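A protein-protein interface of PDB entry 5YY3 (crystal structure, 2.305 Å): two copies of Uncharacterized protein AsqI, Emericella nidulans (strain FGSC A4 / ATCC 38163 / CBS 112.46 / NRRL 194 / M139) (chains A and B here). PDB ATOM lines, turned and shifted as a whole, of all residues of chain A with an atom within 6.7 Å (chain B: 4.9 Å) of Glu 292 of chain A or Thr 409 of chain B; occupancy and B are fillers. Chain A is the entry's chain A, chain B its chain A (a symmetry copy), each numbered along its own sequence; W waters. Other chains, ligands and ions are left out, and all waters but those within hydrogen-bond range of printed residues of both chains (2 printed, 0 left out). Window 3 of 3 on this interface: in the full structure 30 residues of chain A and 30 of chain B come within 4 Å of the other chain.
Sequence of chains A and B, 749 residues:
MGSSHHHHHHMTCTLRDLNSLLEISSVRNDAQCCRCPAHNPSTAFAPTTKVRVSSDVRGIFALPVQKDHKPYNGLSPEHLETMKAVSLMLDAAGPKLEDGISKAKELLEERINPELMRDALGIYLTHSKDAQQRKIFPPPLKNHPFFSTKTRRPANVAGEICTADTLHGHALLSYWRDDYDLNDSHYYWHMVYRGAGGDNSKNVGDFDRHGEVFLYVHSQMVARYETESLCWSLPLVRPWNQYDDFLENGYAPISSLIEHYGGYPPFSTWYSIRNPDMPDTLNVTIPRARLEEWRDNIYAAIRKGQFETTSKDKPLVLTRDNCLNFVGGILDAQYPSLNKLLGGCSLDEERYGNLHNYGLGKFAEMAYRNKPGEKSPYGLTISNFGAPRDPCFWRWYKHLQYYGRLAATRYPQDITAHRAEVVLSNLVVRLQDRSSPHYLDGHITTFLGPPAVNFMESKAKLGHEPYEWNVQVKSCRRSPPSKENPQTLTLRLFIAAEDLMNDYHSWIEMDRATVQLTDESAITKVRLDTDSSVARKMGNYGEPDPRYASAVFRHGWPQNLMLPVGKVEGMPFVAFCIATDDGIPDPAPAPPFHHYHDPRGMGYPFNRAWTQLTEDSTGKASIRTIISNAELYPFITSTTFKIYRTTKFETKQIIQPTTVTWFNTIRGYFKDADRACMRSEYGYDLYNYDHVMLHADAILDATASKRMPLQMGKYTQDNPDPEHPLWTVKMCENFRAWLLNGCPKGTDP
Among the printed residues, pairs that only touch across the chains: Gln 242 of chain A with Arg 405 of chain B (3.9 Å), Glu 292 of chain A with Arg 303 of chain B (3.97 Å), Glu 292 of chain A with Thr 409 of chain B (3.9 Å), Glu 293 of chain A with Arg 303 of chain B (3.4 Å), Arg 295 of chain A with Leu 406 of chain B (3.4 Å) and Asn 297 of chain A with Arg 303 of chain B (3.9 Å).
The side-chain carboxylate (OD2) of Asp 244 of chain A lies within salt-bridge range of the guanidinium group (NH1) of Arg 405 of chain B (2.8 Å).
The guanidinium group (NH2) of Arg 303 of chain B is in salt-bridge range of the side-chain carboxylate (OD2) of Asp 296 of chain A (2.8 Å).
No position is printed for both chains.
Of the 8 pairs that touch across the chains among the printed residues, none has its exchanged pair printed and touching as well.
Of the 11 printed residues of chain B, 4 touch a printed residue of chain A.
Printed residues of chain B that touch a printed residue of chain A: Arg 303, Arg 405, Leu 406 and Thr 409.
Hydrophobic or aromatic side chains of chain B that line the printed part of chain A: Leu 406.
Among the printed residues, Asp or Glu carboxylates within 4 Å of a Lys or Arg side-chain nitrogen of the other chain: Asp 244 of chain A with Arg 405 of chain B (2.8 Å) and Asp 296 of chain A with Arg 303 of chain B (2.8 Å).
NH1 of Arg 290 of chain A lies within salt-bridge range of OE1 of Glu 293 of chain A, 3.0 Å away.
The guanidinium group (NH2) of Arg 295 of chain A is in salt-bridge range of the side-chain carboxylate (OD1) of Asp 296 of chain A (3.1 Å).
The guanidinium group (NE) of Arg 288 of chain A is in salt-bridge range of the side-chain carboxylate (OE2) of Glu 292 of chain A (3.9 Å).
The backbone carbonyl oxygen (O) of Arg 303 of chain B is in hydrogen-bond range of the guanidinium group (NH2) of Arg 410 of chain B, at 3.0 Å.
O of Glu 293 of chain A lies close to ND2 of Asn 297 of chain A, at 3.4 Å.
Printed residues of chain B within 4 Å of Gln 242 of chain A: Arg 405 (3.9 Å).
Pro 287 of chain A touches none of the printed residues of chain B.
Glu 292 of chain A touches just these residues of chain B: Arg 303 and Thr 409.
Of the printed residues of chain B, Asp 296 of chain A touches Arg 303.
Of the printed residues of chain B, Asn 297 of chain A touches Arg 303.
Of the printed residues of chain A, Arg 303 of chain B touches Glu 292 (3.97 Å), Glu 293 (3.4 Å), Asp 296 (2.8 Å) and Asn 297 (3.9 Å).
Printed residues of chain A within 4 Å of Leu 406 of chain B: Arg 295.
Thr 409 of chain B touches just one residue of chain A: Glu 292 (3.9 Å).
The nearest printed residue of chain B that does not touch Gln 242 of chain A is Leu 406 of chain B (7.6 Å).
Water W1 lies within hydrogen-bond range of OE1 of Glu 292 of chain A (2.8 Å), NH2 of Arg 303 of chain B (3.1 Å) and OG1 of Thr 409 of chain B (3.4 Å).
Water W2 bridges NE of Arg 405 of chain B and OE1 of Gln 242 of chain A.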
ATOM      1  N   GLN A 242      18.922 -14.279  16.080  1.00  0.00           N
ATOM      2  CA  GLN A 242      17.507 -13.951  16.040  1.00  0.00           C
ATOM      3  C   GLN A 242      17.355 -12.420  15.963  1.00  0.00           C
ATOM      4  O   GLN A 242      17.754 -11.698  16.874  1.00  0.00           O
ATOM      5  CB  GLN A 242      16.788 -14.543  17.273  1.00  0.00           C
ATOM      6  CG  GLN A 242      17.032 -16.063  17.479  1.00  0.00           C
ATOM      7  CD  GLN A 242      16.299 -16.665  18.704  1.00  0.00           C
ATOM      8  OE1 GLN A 242      15.661 -15.950  19.494  1.00  0.00           O
ATOM      9  NE2 GLN A 242      16.417 -17.991  18.873  1.00  0.00           N
ATOM     10  N   TYR A 243      16.795 -11.920  14.870  1.00  0.00           N
ATOM     11  CA  TYR A 243      16.816 -10.474  14.610  1.00  0.00           C
ATOM     12  C   TYR A 243      15.752  -9.695  15.402  1.00  0.00           C
ATOM     13  O   TYR A 243      15.749  -8.463  15.403  1.00  0.00           O
ATOM     14  CB  TYR A 243      16.648 -10.191  13.103  1.00  0.00           C
ATOM     15  CG  TYR A 243      17.763 -10.712  12.226  1.00  0.00           C
ATOM     16  CD1 TYR A 243      18.921 -11.260  12.782  1.00  0.00           C
ATOM     17  CD2 TYR A 243      17.653 -10.672  10.826  1.00  0.00           C
ATOM     18  CE1 TYR A 243      19.943 -11.752  11.972  1.00  0.00           C
ATOM     19  CE2 TYR A 243      18.671 -11.160  10.006  1.00  0.00           C
ATOM     20  CZ  TYR A 243      19.813 -11.692  10.590  1.00  0.00           C
ATOM     21  OH  TYR A 243      20.831 -12.171   9.800  1.00  0.00           O
ATOM     22  N   ASP A 244      14.852 -10.410  16.070  1.00  0.00           N
ATOM     23  CA  ASP A 244      13.884  -9.782  16.959  1.00  0.00           C
ATOM     24  C   ASP A 244      14.377  -9.803  18.399  1.00  0.00           C
ATOM     25  O   ASP A 244      13.591  -9.829  19.343  1.00  0.00           O
ATOM     26  CB  ASP A 244      12.533 -10.487  16.856  1.00  0.00           C
ATOM     27  CG  ASP A 244      12.634 -11.971  17.170  1.00  0.00           C
ATOM     28  OD1 ASP A 244      13.768 -12.509  17.121  1.00  0.00           O
ATOM     29  OD2 ASP A 244      11.586 -12.603  17.448  1.00  0.00           O
ATOM     30  N   TRP A 270      16.041  -3.773  17.081  1.00  0.00           N
ATOM     31  CA  TRP A 270      15.847  -3.286  15.715  1.00  0.00           C
ATOM     32  C   TRP A 270      14.426  -2.753  15.585  1.00  0.00           C
ATOM     33  O   TRP A 270      13.519  -3.181  16.318  1.00  0.00           O
ATOM     34  CB  TRP A 270      16.076  -4.385  14.681  1.00  0.00           C
ATOM     35  CG  TRP A 270      17.525  -4.699  14.387  1.00  0.00           C
ATOM     36  CD1 TRP A 270      18.625  -4.200  15.017  1.00  0.00           C
ATOM     37  CD2 TRP A 270      18.007  -5.580  13.368  1.00  0.00           C
ATOM     38  NE1 TRP A 270      19.769  -4.717  14.449  1.00  0.00           N
ATOM     39  CE2 TRP A 270      19.413  -5.572  13.438  1.00  0.00           C
ATOM     40  CE3 TRP A 270      17.383  -6.385  12.407  1.00  0.00           C
ATOM     41  CZ2 TRP A 270      20.213  -6.329  12.570  1.00  0.00           C
ATOM     42  CZ3 TRP A 270      18.173  -7.139  11.555  1.00  0.00           C
ATOM     43  CH2 TRP A 270      19.576  -7.111  11.643  1.00  0.00           C
ATOM     44  N   PRO A 287      12.902  -3.481   6.275  1.00  0.00           N
ATOM     45  CA  PRO A 287      12.271  -4.099   7.445  1.00  0.00           C
ATOM     46  C   PRO A 287      13.042  -5.332   7.919  1.00  0.00           C
ATOM     47  O   PRO A 287      13.709  -5.992   7.126  1.00  0.00           O
ATOM     48  CB  PRO A 287      10.859  -4.460   6.946  1.00  0.00           C
ATOM     49  CG  PRO A 287      10.930  -4.422   5.461  1.00  0.00           C
ATOM     50  CD  PRO A 287      12.053  -3.516   5.072  1.00  0.00           C
ATOM     51  N   ARG A 288      12.968  -5.605   9.214  1.00  0.00           N
ATOM     52  CA  ARG A 288      13.591  -6.777   9.800  1.00  0.00           C
ATOM     53  C   ARG A 288      13.336  -8.049   8.982  1.00  0.00           C
ATOM     54  O   ARG A 288      14.248  -8.867   8.780  1.00  0.00           O
ATOM     55  CB  ARG A 288      13.094  -6.974  11.231  1.00  0.00           C
ATOM     56  CG  ARG A 288      13.733  -8.165  11.913  1.00  0.00           C
ATOM     57  CD  ARG A 288      13.155  -8.347  13.303  1.00  0.00           C
ATOM     58  NE  ARG A 288      11.723  -8.593  13.218  1.00  0.00           N
ATOM     59  CZ  ARG A 288      10.805  -8.001  13.977  1.00  0.00           C
ATOM     60  NH1 ARG A 288      11.168  -7.114  14.914  1.00  0.00           N
ATOM     61  NH2 ARG A 288       9.522  -8.308  13.803  1.00  0.00           N
ATOM     62  N   ALA A 289      12.102  -8.213   8.508  1.00  0.00           N
ATOM     63  CA  ALA A 289      11.707  -9.422   7.768  1.00  0.00           C
ATOM     64  C   ALA A 289      12.524  -9.613   6.488  1.00  0.00           C
ATOM     65  O   ALA A 289      12.822 -10.741   6.084  1.00  0.00           O
ATOM     66  CB  ALA A 289      10.222  -9.375   7.441  1.00  0.00           C
ATOM     67  N   ARG A 290      12.897  -8.501   5.869  1.00  0.00           N
ATOM     68  CA  ARG A 290      13.685  -8.497   4.644  1.00  0.00           C
ATOM     69  C   ARG A 290      15.112  -9.035   4.918  1.00  0.00           C
ATOM     70  O   ARG A 290      15.673  -9.784   4.112  1.00  0.00           O
ATOM     71  CB  ARG A 290      13.728  -7.073   4.073  1.00  0.00           C
ATOM     72  CG  ARG A 290      14.462  -6.909   2.755  1.00  0.00           C
ATOM     73  CD  ARG A 290      13.760  -7.641   1.629  1.00  0.00           C
ATOM     74  NE  ARG A 290      14.514  -7.537   0.379  1.00  0.00           N
ATOM     75  CZ  ARG A 290      14.500  -8.464  -0.579  1.00  0.00           C
ATOM     76  NH1 ARG A 290      13.780  -9.573  -0.428  1.00  0.00           N
ATOM     77  NH2 ARG A 290      15.229  -8.301  -1.675  1.00  0.00           N
ATOM     78  N   LEU A 291      15.685  -8.662   6.062  1.00  0.00           N
ATOM     79  CA  LEU A 291      17.013  -9.146   6.434  1.00  0.00           C
ATOM     80  C   LEU A 291      16.956 -10.634   6.776  1.00  0.00           C
ATOM     81  O   LEU A 291      17.821 -11.408   6.360  1.00  0.00           O
ATOM     82  CB  LEU A 291      17.575  -8.345   7.608  1.00  0.00           C
ATOM     83  CG  LEU A 291      17.923  -6.897   7.260  1.00  0.00           C
ATOM     84  CD1 LEU A 291      17.118  -5.953   8.127  1.00  0.00           C
ATOM     85  CD2 LEU A 291      19.391  -6.637   7.433  1.00  0.00           C
ATOM     86  N   GLU A 292      15.916 -11.027   7.511  1.00  0.00           N
ATOM     87  CA  GLU A 292      15.716 -12.426   7.880  1.00  0.00           C
ATOM     88  C   GLU A 292      15.633 -13.316   6.633  1.00  0.00           C
ATOM     89  O   GLU A 292      16.213 -14.403   6.592  1.00  0.00           O
ATOM     90  CB  GLU A 292      14.448 -12.574   8.735  1.00  0.00           C
ATOM     91  CG  GLU A 292      14.458 -11.733  10.001  1.00  0.00           C
ATOM     92  CD  GLU A 292      13.229 -11.925  10.860  1.00  0.00           C
ATOM     93  OE1 GLU A 292      12.136 -12.072  10.282  1.00  0.00           O
ATOM     94  OE2 GLU A 292      13.351 -11.919  12.110  1.00  0.00           O
ATOM     95  N   GLU A 293      14.920 -12.849   5.614  1.00  0.00           N
ATOM     96  CA  GLU A 293      14.801 -13.605   4.365  1.00  0.00           C
ATOM     97  C   GLU A 293      16.172 -13.860   3.699  1.00  0.00           C
ATOM     98  O   GLU A 293      16.500 -15.002   3.367  1.00  0.00           O
ATOM     99  CB  GLU A 293      13.867 -12.880   3.409  1.00  0.00           C
ATOM    100  CG  GLU A 293      13.954 -13.398   1.996  1.00  0.00           C
ATOM    101  CD  GLU A 293      12.863 -12.848   1.102  1.00  0.00           C
ATOM    102  OE1 GLU A 293      12.494 -11.662   1.269  1.00  0.00           O
ATOM    103  OE2 GLU A 293      12.381 -13.616   0.236  1.00  0.00           O
ATOM    104  N   TRP A 294      16.967 -12.802   3.534  1.00  0.00           N
ATOM    105  CA  TRP A 294      18.361 -12.917   3.088  1.00  0.00           C
ATOM    106  C   TRP A 294      19.149 -13.954   3.903  1.00  0.00           C
ATOM    107  O   TRP A 294      19.790 -14.843   3.337  1.00  0.00           O
ATOM    108  CB  TRP A 294      19.060 -11.550   3.178  1.00  0.00           C
ATOM    109  CG  TRP A 294      18.566 -10.537   2.170  1.00  0.00           C
ATOM    110  CD1 TRP A 294      17.908 -10.802   1.003  1.00  0.00           C
ATOM    111  CD2 TRP A 294      18.700  -9.107   2.242  1.00  0.00           C
ATOM    112  NE1 TRP A 294      17.625  -9.630   0.342  1.00  0.00           N
ATOM    113  CE2 TRP A 294      18.096  -8.575   1.076  1.00  0.00           C
ATOM    114  CE3 TRP A 294      19.271  -8.226   3.170  1.00  0.00           C
ATOM    115  CZ2 TRP A 294      18.048  -7.197   0.816  1.00  0.00           C
ATOM    116  CZ3 TRP A 294      19.226  -6.853   2.912  1.00  0.00           C
ATOM    117  CH2 TRP A 294      18.616  -6.353   1.744  1.00  0.00           C
ATOM    118  N   ARG A 295      19.087 -13.830   5.228  1.00  0.00           N
ATOM    119  CA  ARG A 295      19.721 -14.774   6.151  1.00  0.00           C
ATOM    120  C   ARG A 295      19.267 -16.205   5.876  1.00  0.00           C
ATOM    121  O   ARG A 295      20.089 -17.118   5.803  1.00  0.00           O
ATOM    122  CB  ARG A 295      19.400 -14.408   7.608  1.00  0.00           C
ATOM    123  CG  ARG A 295      19.828 -15.462   8.637  1.00  0.00           C
ATOM    124  CD  ARG A 295      19.070 -15.286   9.948  1.00  0.00           C
ATOM    125  NE  ARG A 295      17.675 -15.675   9.785  1.00  0.00           N
ATOM    126  CZ  ARG A 295      16.684 -15.333  10.606  1.00  0.00           C
ATOM    127  NH1 ARG A 295      16.932 -14.568  11.661  1.00  0.00           N
ATOM    128  NH2 ARG A 295      15.436 -15.747  10.364  1.00  0.00           N
ATOM    129  N   ASP A 296      17.952 -16.388   5.758  1.00  0.00           N
ATOM    130  CA  ASP A 296      17.373 -17.712   5.532  1.00  0.00           C
ATOM    131  C   ASP A 296      17.879 -18.301   4.227  1.00  0.00           C
ATOM    132  O   ASP A 296      18.086 -19.511   4.114  1.00  0.00           O
ATOM    133  CB  ASP A 296      15.846 -17.651   5.481  1.00  0.00           C
ATOM    134  CG  ASP A 296      15.228 -17.349   6.811  1.00  0.00           C
ATOM    135  OD1 ASP A 296      15.945 -17.463   7.834  1.00  0.00           O
ATOM    136  OD2 ASP A 296      14.014 -17.014   6.833  1.00  0.00           O
ATOM    137  N   ASN A 297      18.058 -17.436   3.234  1.00  0.00           N
ATOM    138  CA  ASN A 297      18.452 -17.896   1.915  1.00  0.00           C
ATOM    139  C   ASN A 297      19.932 -18.269   1.900  1.00  0.00           C
ATOM    140  O   ASN A 297      20.317 -19.277   1.302  1.00  0.00           O
ATOM    141  CB  ASN A 297      18.135 -16.831   0.860  1.00  0.00           C
ATOM    142  CG  ASN A 297      16.642 -16.691   0.601  1.00  0.00           C
ATOM    143  OD1 ASN A 297      15.860 -17.579   0.932  1.00  0.00           O
ATOM    144  ND2 ASN A 297      16.246 -15.581  -0.007  1.00  0.00           N
ATOM    145  N   TYR A 299      21.470 -19.270   4.557  1.00  0.00           N
ATOM    146  CA  TYR A 299      21.496 -20.515   5.329  1.00  0.00           C
ATOM    147  C   TYR A 299      21.224 -21.709   4.414  1.00  0.00           C
ATOM    148  O   TYR A 299      21.962 -22.707   4.408  1.00  0.00           O
ATOM    149  CB  TYR A 299      20.461 -20.500   6.448  1.00  0.00           C
ATOM    150  CG  TYR A 299      20.805 -19.683   7.687  1.00  0.00           C
ATOM    151  CD1 TYR A 299      22.064 -19.124   7.870  1.00  0.00           C
ATOM    152  CD2 TYR A 299      19.853 -19.487   8.681  1.00  0.00           C
ATOM    153  CE1 TYR A 299      22.358 -18.376   9.011  1.00  0.00           C
ATOM    154  CE2 TYR A 299      20.142 -18.763   9.815  1.00  0.00           C
ATOM    155  CZ  TYR A 299      21.394 -18.210   9.981  1.00  0.00           C
ATOM    156  OH  TYR A 299      21.645 -17.478  11.123  1.00  0.00           O
ATOM    157  N   LEU A 355      23.364  -8.480   3.429  1.00  0.00           N
ATOM    158  CA  LEU A 355      22.981  -8.682   4.832  1.00  0.00           C
ATOM    159  C   LEU A 355      23.887  -7.990   5.860  1.00  0.00           C
ATOM    160  O   LEU A 355      23.390  -7.430   6.836  1.00  0.00           O
ATOM    161  CB  LEU A 355      22.928 -10.179   5.144  1.00  0.00           C
ATOM    162  CG  LEU A 355      22.429 -10.584   6.524  1.00  0.00           C
ATOM    163  CD1 LEU A 355      21.097  -9.917   6.808  1.00  0.00           C
ATOM    164  CD2 LEU A 355      22.293 -12.084   6.595  1.00  0.00           C
ATOM    165  N   ARG B 303      10.997 -21.194   5.557  1.00  0.00           N
ATOM    166  CA  ARG B 303      11.173 -20.055   4.671  1.00  0.00           C
ATOM    167  C   ARG B 303      10.504 -20.322   3.313  1.00  0.00           C
ATOM    168  O   ARG B 303       9.843 -19.446   2.750  1.00  0.00           O
ATOM    169  CB  ARG B 303      12.664 -19.750   4.488  1.00  0.00           C
ATOM    170  CG  ARG B 303      13.018 -18.915   3.254  1.00  0.00           C
ATOM    171  CD  ARG B 303      12.316 -17.562   3.223  1.00  0.00           C
ATOM    172  NE  ARG B 303      12.559 -16.804   4.443  1.00  0.00           N
ATOM    173  CZ  ARG B 303      11.863 -15.730   4.817  1.00  0.00           C
ATOM    174  NH1 ARG B 303      10.862 -15.279   4.065  1.00  0.00           N
ATOM    175  NH2 ARG B 303      12.166 -15.117   5.956  1.00  0.00           N
ATOM    176  N   ARG B 405       9.080 -18.753  16.453  1.00  0.00           N
ATOM    177  CA  ARG B 405       9.278 -17.374  16.010  1.00  0.00           C
ATOM    178  C   ARG B 405       9.326 -17.265  14.486  1.00  0.00           C
ATOM    179  O   ARG B 405       8.740 -16.341  13.910  1.00  0.00           O
ATOM    180  CB  ARG B 405      10.557 -16.787  16.608  1.00  0.00           C
ATOM    181  CG  ARG B 405      10.523 -16.686  18.123  1.00  0.00           C
ATOM    182  CD  ARG B 405      11.825 -16.112  18.675  1.00  0.00           C
ATOM    183  NE  ARG B 405      11.736 -15.941  20.121  1.00  0.00           N
ATOM    184  CZ  ARG B 405      11.340 -14.818  20.695  1.00  0.00           C
ATOM    185  NH1 ARG B 405      10.995 -13.788  19.933  1.00  0.00           N
ATOM    186  NH2 ARG B 405      11.263 -14.732  22.015  1.00  0.00           N
ATOM    187  N   LEU B 406      10.026 -18.199  13.839  1.00  0.00           N
ATOM    188  CA  LEU B 406      10.151 -18.201  12.381  1.00  0.00           C
ATOM    189  C   LEU B 406       8.785 -18.343  11.705  1.00  0.00           C
ATOM    190  O   LEU B 406       8.455 -17.615  10.762  1.00  0.00           O
ATOM    191  CB  LEU B 406      11.061 -19.333  11.917  1.00  0.00           C
ATOM    192  CG  LEU B 406      12.557 -19.164  12.198  1.00  0.00           C
ATOM    193  CD1 LEU B 406      13.247 -20.509  12.103  1.00  0.00           C
ATOM    194  CD2 LEU B 406      13.192 -18.168  11.224  1.00  0.00           C
ATOM    195  N   ALA B 407       7.999 -19.292  12.187  1.00  0.00           N
ATOM    196  CA  ALA B 407       6.721 -19.591  11.563  1.00  0.00           C
ATOM    197  C   ALA B 407       5.762 -18.433  11.805  1.00  0.00           C
ATOM    198  O   ALA B 407       5.070 -17.983  10.886  1.00  0.00           O
ATOM    199  CB  ALA B 407       6.146 -20.905  12.104  1.00  0.00           C
ATOM    200  N   ALA B 408       5.768 -17.931  13.039  1.00  0.00           N
ATOM    201  CA  ALA B 408       4.856 -16.878  13.446  1.00  0.00           C
ATOM    202  C   ALA B 408       5.022 -15.601  12.620  1.00  0.00           C
ATOM    203  O   ALA B 408       4.030 -14.967  12.266  1.00  0.00           O
ATOM    204  CB  ALA B 408       5.038 -16.575  14.933  1.00  0.00           C
ATOM    205  N   THR B 409       6.253 -15.195  12.314  1.00  0.00           N
ATOM    206  CA  THR B 409       6.388 -13.967  11.526  1.00  0.00           C
ATOM    207  C   THR B 409       6.132 -14.225  10.027  1.00  0.00           C
ATOM    208  O   THR B 409       5.811 -13.289   9.277  1.00  0.00           O
ATOM    209  CB  THR B 409       7.770 -13.304  11.693  1.00  0.00           C
ATOM    210  OG1 THR B 409       8.716 -13.904  10.801  1.00  0.00           O
ATOM    211  CG2 THR B 409       8.256 -13.417  13.118  1.00  0.00           C
ATOM    212  N   ARG B 410       6.271 -15.486   9.605  1.00  0.00           N
ATOM    213  CA  ARG B 410       5.977 -15.889   8.223  1.00  0.00           C
ATOM    214  C   ARG B 410       4.480 -15.897   7.881  1.00  0.00           C
ATOM    215  O   ARG B 410       4.104 -15.595   6.751  1.00  0.00           O
ATOM    216  CB  ARG B 410       6.568 -17.278   7.939  1.00  0.00           C
ATOM    217  CG  ARG B 410       8.021 -17.237   7.504  1.00  0.00           C
ATOM    218  CD  ARG B 410       8.173 -16.810   6.054  1.00  0.00           C
ATOM    219  NE  ARG B 410       7.902 -17.926   5.153  1.00  0.00           N
ATOM    220  CZ  ARG B 410       7.101 -17.854   4.098  1.00  0.00           C
ATOM    221  NH1 ARG B 410       6.477 -16.719   3.817  1.00  0.00           N
ATOM    222  NH2 ARG B 410       6.908 -18.921   3.337  1.00  0.00           N
ATOM    223  N   TYR B 411       3.634 -16.241   8.850  1.00  0.00           N
ATOM    224  CA  TYR B 411       2.194 -16.290   8.626  1.00  0.00           C
ATOM    225  C   TYR B 411       1.434 -15.441   9.631  1.00  0.00           C
ATOM    226  O   TYR B 411       0.841 -15.970  10.580  1.00  0.00           O
ATOM    227  CB  TYR B 411       1.705 -17.743   8.663  1.00  0.00           C
ATOM    228  CG  TYR B 411       2.406 -18.587   7.618  1.00  0.00           C
ATOM    229  CD1 TYR B 411       2.052 -18.500   6.276  1.00  0.00           C
ATOM    230  CD2 TYR B 411       3.454 -19.428   7.965  1.00  0.00           C
ATOM    231  CE1 TYR B 411       2.717 -19.246   5.311  1.00  0.00           C
ATOM    232  CE2 TYR B 411       4.121 -20.178   7.007  1.00  0.00           C
ATOM    233  CZ  TYR B 411       3.746 -20.080   5.687  1.00  0.00           C
ATOM    234  OH  TYR B 411       4.406 -20.822   4.744  1.00  0.00           O
ATOM    235  N   PRO B 412       1.437 -14.112   9.415  1.00  0.00           N
ATOM    236  CA  PRO B 412       0.816 -13.147  10.328  1.00  0.00           C
ATOM    237  C   PRO B 412      -0.694 -13.363  10.415  1.00  0.00           C
ATOM    238  O   PRO B 412      -1.242 -14.125   9.624  1.00  0.00           O
ATOM    239  CB  PRO B 412       1.132 -11.785   9.696  1.00  0.00           C
ATOM    240  CG  PRO B 412       2.163 -12.037   8.659  1.00  0.00           C
ATOM    241  CD  PRO B 412       2.089 -13.466   8.264  1.00  0.00           C
ATOM    242  N   ALA B 609       2.423 -13.529  14.149  1.00  0.00           N
ATOM    243  CA  ALA B 609       2.671 -12.096  14.071  1.00  0.00           C
ATOM    244  C   ALA B 609       1.352 -11.398  13.748  1.00  0.00           C
ATOM    245  O   ALA B 609       0.424 -12.034  13.246  1.00  0.00           O
ATOM    246  CB  ALA B 609       3.726 -11.770  13.028  1.00  0.00           C
ATOM    247  N   THR B 614       3.179  -6.236  10.759  1.00  0.00           N
ATOM    248  CA  THR B 614       3.993  -6.678   9.626  1.00  0.00           C
ATOM    249  C   THR B 614       3.747  -5.828   8.381  1.00  0.00           C
ATOM    250  O   THR B 614       4.638  -5.701   7.533  1.00  0.00           O
ATOM    251  CB  THR B 614       3.749  -8.152   9.267  1.00  0.00           C
ATOM    252  OG1 THR B 614       2.359  -8.353   8.997  1.00  0.00           O
ATOM    253  CG2 THR B 614       4.176  -9.061  10.419  1.00  0.00           C
HETATM  254  O   HOH W   1      10.791 -13.320   8.146  1.00  0.00           O
HETATM  255  O   HOH W   2      13.780 -18.039  20.540  1.00  0.00           O
